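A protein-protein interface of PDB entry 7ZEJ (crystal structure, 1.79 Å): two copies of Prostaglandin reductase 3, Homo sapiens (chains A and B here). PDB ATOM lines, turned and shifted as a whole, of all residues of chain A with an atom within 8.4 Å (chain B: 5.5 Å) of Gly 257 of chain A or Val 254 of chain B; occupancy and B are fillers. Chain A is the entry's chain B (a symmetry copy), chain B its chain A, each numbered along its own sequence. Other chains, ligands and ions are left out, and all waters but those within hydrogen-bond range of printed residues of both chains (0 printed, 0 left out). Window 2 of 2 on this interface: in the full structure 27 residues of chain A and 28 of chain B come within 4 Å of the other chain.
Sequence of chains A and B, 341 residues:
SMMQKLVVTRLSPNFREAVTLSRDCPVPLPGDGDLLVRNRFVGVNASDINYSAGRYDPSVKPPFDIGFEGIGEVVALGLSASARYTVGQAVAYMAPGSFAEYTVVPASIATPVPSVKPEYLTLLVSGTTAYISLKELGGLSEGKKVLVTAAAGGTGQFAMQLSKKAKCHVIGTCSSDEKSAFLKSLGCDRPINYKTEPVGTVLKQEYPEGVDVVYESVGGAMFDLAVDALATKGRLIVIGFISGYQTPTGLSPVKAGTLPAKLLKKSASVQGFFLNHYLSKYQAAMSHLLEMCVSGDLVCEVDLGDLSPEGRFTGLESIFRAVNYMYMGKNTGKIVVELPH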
ATOM      1  N   ASP A 224      18.160  29.036  -2.892  1.00  0.00           N
ATOM      2  CA  ASP A 224      18.100  27.564  -2.721  1.00  0.00           C
ATOM      3  C   ASP A 224      19.170  26.924  -3.612  1.00  0.00           C
ATOM      4  O   ASP A 224      19.807  25.970  -3.209  1.00  0.00           O
ATOM      5  CB  ASP A 224      16.724  27.022  -3.118  1.00  0.00           C
ATOM      6  CG  ASP A 224      15.603  27.457  -2.203  1.00  0.00           C
ATOM      7  OD1 ASP A 224      15.865  27.710  -0.985  1.00  0.00           O
ATOM      8  OD2 ASP A 224      14.465  27.534  -2.711  1.00  0.00           O
ATOM      9  N   VAL A 254      12.111  30.215   1.094  1.00  0.00           N
ATOM     10  CA  VAL A 254      13.317  29.368   0.849  1.00  0.00           C
ATOM     11  C   VAL A 254      13.117  27.955   1.426  1.00  0.00           C
ATOM     12  O   VAL A 254      12.394  27.796   2.402  1.00  0.00           O
ATOM     13  CB  VAL A 254      14.582  30.041   1.416  1.00  0.00           C
ATOM     14  CG1 VAL A 254      14.941  31.317   0.651  1.00  0.00           C
ATOM     15  CG2 VAL A 254      14.446  30.307   2.911  1.00  0.00           C
ATOM     16  N   LYS A 255      13.793  26.962   0.853  1.00  0.00           N
ATOM     17  CA  LYS A 255      13.848  25.575   1.388  1.00  0.00           C
ATOM     18  C   LYS A 255      14.805  25.567   2.578  1.00  0.00           C
ATOM     19  O   LYS A 255      15.994  25.295   2.403  1.00  0.00           O
ATOM     20  CB  LYS A 255      14.288  24.598   0.299  1.00  0.00           C
ATOM     21  CG  LYS A 255      13.254  24.369  -0.798  1.00  0.00           C
ATOM     22  CD  LYS A 255      13.711  23.400  -1.858  1.00  0.00           C
ATOM     23  CE  LYS A 255      12.713  23.339  -2.993  1.00  0.00           C
ATOM     24  NZ  LYS A 255      12.948  22.176  -3.879  1.00  0.00           N
ATOM     25  N   ALA A 256      14.287  25.883   3.748  1.00  0.00           N
ATOM     26  CA  ALA A 256      15.070  26.129   4.976  1.00  0.00           C
ATOM     27  C   ALA A 256      15.098  24.898   5.892  1.00  0.00           C
ATOM     28  O   ALA A 256      16.003  24.820   6.714  1.00  0.00           O
ATOM     29  CB  ALA A 256      14.469  27.315   5.694  1.00  0.00           C
ATOM     30  N   GLY A 257      14.119  23.995   5.789  1.00  0.00           N
ATOM     31  CA  GLY A 257      13.997  22.843   6.696  1.00  0.00           C
ATOM     32  C   GLY A 257      15.191  21.922   6.571  1.00  0.00           C
ATOM     33  O   GLY A 257      15.601  21.364   7.588  1.00  0.00           O
ATOM     34  N   THR A 258      15.760  21.775   5.372  1.00  0.00           N
ATOM     35  CA  THR A 258      16.943  20.906   5.145  1.00  0.00           C
ATOM     36  C   THR A 258      18.235  21.733   5.121  1.00  0.00           C
ATOM     37  O   THR A 258      19.291  21.142   4.814  1.00  0.00           O
ATOM     38  CB  THR A 258      16.789  20.109   3.849  1.00  0.00           C
ATOM     39  OG1 THR A 258      16.689  21.041   2.779  1.00  0.00           O
ATOM     40  CG2 THR A 258      15.569  19.215   3.844  1.00  0.00           C
ATOM     41  N   LEU A 259      18.192  23.025   5.448  1.00  0.00           N
ATOM     42  CA  LEU A 259      19.391  23.885   5.315  1.00  0.00           C
ATOM     43  C   LEU A 259      20.454  23.483   6.345  1.00  0.00           C
ATOM     44  O   LEU A 259      21.603  23.285   5.976  1.00  0.00           O
ATOM     45  CB  LEU A 259      19.001  25.353   5.467  1.00  0.00           C
ATOM     46  CG  LEU A 259      20.158  26.351   5.378  1.00  0.00           C
ATOM     47  CD1 LEU A 259      20.922  26.199   4.085  1.00  0.00           C
ATOM     48  CD2 LEU A 259      19.635  27.760   5.503  1.00  0.00           C
ATOM     49  N   PRO A 260      20.152  23.385   7.660  1.00  0.00           N
ATOM     50  CA  PRO A 260      21.192  23.018   8.633  1.00  0.00           C
ATOM     51  C   PRO A 260      21.890  21.690   8.304  1.00  0.00           C
ATOM     52  O   PRO A 260      23.084  21.591   8.519  1.00  0.00           O
ATOM     53  CB  PRO A 260      20.450  22.933   9.975  1.00  0.00           C
ATOM     54  CG  PRO A 260      19.239  23.846   9.758  1.00  0.00           C
ATOM     55  CD  PRO A 260      18.858  23.670   8.297  1.00  0.00           C
ATOM     56  N   ALA A 261      21.146  20.710   7.786  1.00  0.00           N
ATOM     57  CA  ALA A 261      21.708  19.415   7.338  1.00  0.00           C
ATOM     58  C   ALA A 261      22.661  19.631   6.159  1.00  0.00           C
ATOM     59  O   ALA A 261      23.768  19.023   6.175  1.00  0.00           O
ATOM     60  CB  ALA A 261      20.610  18.433   6.998  1.00  0.00           C
ATOM     61  N   LYS A 262      22.270  20.423   5.147  1.00  0.00           N
ATOM     62  CA  LYS A 262      23.145  20.669   3.972  1.00  0.00           C
ATOM     63  C   LYS A 262      24.435  21.364   4.429  1.00  0.00           C
ATOM     64  O   LYS A 262      25.480  21.018   3.924  1.00  0.00           O
ATOM     65  CB  LYS A 262      22.437  21.503   2.908  1.00  0.00           C
ATOM     66  CG  LYS A 262      21.389  20.739   2.132  1.00  0.00           C
ATOM     67  CD  LYS A 262      20.587  21.606   1.158  1.00  0.00           C
ATOM     68  CE  LYS A 262      19.456  20.821   0.540  1.00  0.00           C
ATOM     69  NZ  LYS A 262      18.712  21.649  -0.428  1.00  0.00           N
ATOM     70  N   GLY B 219      19.165  20.545  17.528  1.00  0.00           N
ATOM     71  CA  GLY B 219      18.226  20.801  16.410  1.00  0.00           C
ATOM     72  C   GLY B 219      16.810  21.096  16.889  1.00  0.00           C
ATOM     73  O   GLY B 219      16.626  21.286  18.090  1.00  0.00           O
ATOM     74  N   GLY B 220      15.852  21.228  15.961  1.00  0.00           N
ATOM     75  CA  GLY B 220      14.417  21.432  16.253  1.00  0.00           C
ATOM     76  C   GLY B 220      14.166  22.733  16.993  1.00  0.00           C
ATOM     77  O   GLY B 220      14.802  23.768  16.660  1.00  0.00           O
ATOM     78  N   PHE B 223      17.345  24.627  18.183  1.00  0.00           N
ATOM     79  CA  PHE B 223      17.944  25.417  17.075  1.00  0.00           C
ATOM     80  C   PHE B 223      17.195  26.755  16.900  1.00  0.00           C
ATOM     81  O   PHE B 223      17.849  27.820  16.914  1.00  0.00           O
ATOM     82  CB  PHE B 223      17.967  24.597  15.784  1.00  0.00           C
ATOM     83  CG  PHE B 223      18.449  25.332  14.565  1.00  0.00           C
ATOM     84  CD1 PHE B 223      19.803  25.454  14.294  1.00  0.00           C
ATOM     85  CD2 PHE B 223      17.550  25.894  13.672  1.00  0.00           C
ATOM     86  CE1 PHE B 223      20.258  26.105  13.161  1.00  0.00           C
ATOM     87  CE2 PHE B 223      18.006  26.578  12.555  1.00  0.00           C
ATOM     88  CZ  PHE B 223      19.359  26.686  12.299  1.00  0.00           C
ATOM     89  N   ASP B 224      15.871  26.737  16.716  1.00  0.00           N
ATOM     90  CA  ASP B 224      15.065  27.978  16.510  1.00  0.00           C
ATOM     91  C   ASP B 224      15.370  29.014  17.599  1.00  0.00           C
ATOM     92  O   ASP B 224      15.618  30.182  17.309  1.00  0.00           O
ATOM     93  CB  ASP B 224      13.560  27.707  16.568  1.00  0.00           C
ATOM     94  CG  ASP B 224      13.093  26.752  15.494  1.00  0.00           C
ATOM     95  OD1 ASP B 224      13.707  26.753  14.392  1.00  0.00           O
ATOM     96  OD2 ASP B 224      12.122  26.027  15.765  1.00  0.00           O
ATOM     97  N   LEU B 251      16.014  14.231   9.829  1.00  0.00           N
ATOM     98  CA  LEU B 251      15.918  15.704  10.001  1.00  0.00           C
ATOM     99  C   LEU B 251      14.972  16.015  11.167  1.00  0.00           C
ATOM    100  O   LEU B 251      14.043  15.261  11.387  1.00  0.00           O
ATOM    101  CB  LEU B 251      15.421  16.327   8.684  1.00  0.00           C
ATOM    102  CG  LEU B 251      16.167  15.866   7.432  1.00  0.00           C
ATOM    103  CD1 LEU B 251      15.522  16.394   6.154  1.00  0.00           C
ATOM    104  CD2 LEU B 251      17.629  16.277   7.507  1.00  0.00           C
ATOM    105  N   SER B 252      15.196  17.111  11.889  1.00  0.00           N
ATOM    106  CA  SER B 252      14.262  17.665  12.912  1.00  0.00           C
ATOM    107  C   SER B 252      13.549  18.887  12.338  1.00  0.00           C
ATOM    108  O   SER B 252      14.209  19.751  11.778  1.00  0.00           O
ATOM    109  CB  SER B 252      14.989  18.054  14.149  1.00  0.00           C
ATOM    110  OG  SER B 252      14.106  18.051  15.254  1.00  0.00           O
ATOM    111  N   PRO B 253      12.218  19.035  12.494  1.00  0.00           N
ATOM    112  CA  PRO B 253      11.523  20.249  12.047  1.00  0.00           C
ATOM    113  C   PRO B 253      12.049  21.524  12.724  1.00  0.00           C
ATOM    114  O   PRO B 253      12.274  21.544  13.905  1.00  0.00           O
ATOM    115  CB  PRO B 253      10.044  20.012  12.366  1.00  0.00           C
ATOM    116  CG  PRO B 253      10.026  18.831  13.317  1.00  0.00           C
ATOM    117  CD  PRO B 253      11.298  18.043  13.066  1.00  0.00           C
ATOM    118  N   VAL B 254      12.317  22.543  11.908  1.00  0.00           N
ATOM    119  CA  VAL B 254      12.734  23.898  12.362  1.00  0.00           C
ATOM    120  C   VAL B 254      11.756  24.911  11.752  1.00  0.00           C
ATOM    121  O   VAL B 254      11.148  24.583  10.735  1.00  0.00           O
ATOM    122  CB  VAL B 254      14.207  24.161  11.989  1.00  0.00           C
ATOM    123  CG1 VAL B 254      15.160  23.315  12.840  1.00  0.00           C
ATOM    124  CG2 VAL B 254      14.478  23.931  10.506  1.00  0.00           C
ATOM    125  N   LYS B 255      11.541  26.044  12.427  1.00  0.00           N
ATOM    126  CA  LYS B 255      10.720  27.193  11.951  1.00  0.00           C
ATOM    127  C   LYS B 255      11.696  28.209  11.360  1.00  0.00           C
ATOM    128  O   LYS B 255      11.922  29.225  11.993  1.00  0.00           O
ATOM    129  CB  LYS B 255       9.928  27.814  13.111  1.00  0.00           C
ATOM    130  CG  LYS B 255       8.884  26.914  13.753  1.00  0.00           C
ATOM    131  CD  LYS B 255       8.244  27.498  14.990  1.00  0.00           C
ATOM    132  CE  LYS B 255       7.119  26.634  15.525  1.00  0.00           C
ATOM    133  NZ  LYS B 255       6.019  26.499  14.536  1.00  0.00           N
ATOM    134  N   ALA B 256      12.313  27.875  10.232  1.00  0.00           N
ATOM    135  CA  ALA B 256      13.489  28.568   9.679  1.00  0.00           C
ATOM    136  C   ALA B 256      13.166  29.265   8.341  1.00  0.00           C
ATOM    137  O   ALA B 256      14.126  29.678   7.633  1.00  0.00           O
ATOM    138  CB  ALA B 256      14.602  27.552   9.550  1.00  0.00           C
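Ala 256 of chain A touches its own counterpart, Ala 256 of chain B.
Positions printed for both chains: 224, 254, 255 and 256.
Among the printed residues, merely in contact across the chains: Ala 256 of chain A with Ala 256 of chain B (3.1 Å), Thr 258 of chain A with Leu 251 of chain B (3.6 Å), Ala 261 of chain A with Leu 251 of chain B (3.7 Å), Pro 260 of chain A with Phe 223 of chain B (3.8 Å) and Gly 257 of chain A with Val 254 of chain B (3.99 Å).
Hydrophobic or aromatic side chains of chain B within 4 Å of the printed part of chain A: Phe 223, Leu 251, Val 254 and Ala 256.
Of the 10 printed residues of chain A, 5 touch a printed residue of chain B.
Printed residues of chain A that touch a printed residue of chain B: Ala 256, Gly 257, Thr 258, Pro 260 and Ala 261.
Among the printed residues, no Asp or Glu carboxylate lies within 4 Å of a Lys or Arg side-chain nitrogen of the other chain.
Printed residues of chain B within 4 Å of Ala 256 of chain A: Ala 256.
Of the printed residues of chain B, Gly 257 of chain A touches Val 254.
Printed residues of chain B within 4 Å of Thr 258 of chain A: Leu 251 (3.6 Å).
Printed residues of chain B within 4 Å of Pro 260 of chain A: Phe 223 (3.8 Å).
Printed residues of chain A within 4 Å of Leu 251 of chain B: Thr 258 and Ala 261.
Of the printed residues of chain A, Val 254 of chain B touches Gly 257 (3.99 Å).
The nearest printed residue of chain B that does not touch Gly 257 of chain A is Ser 252 of chain B (4.7 Å).
The nearest printed residue of chain A that does not touch Val 254 of chain B is Ala 256 of chain A (4.2 Å).
The nearest printed residue of chain A that does not touch Leu 251 of chain B is Gly 257 of chain A (5.2 Å).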
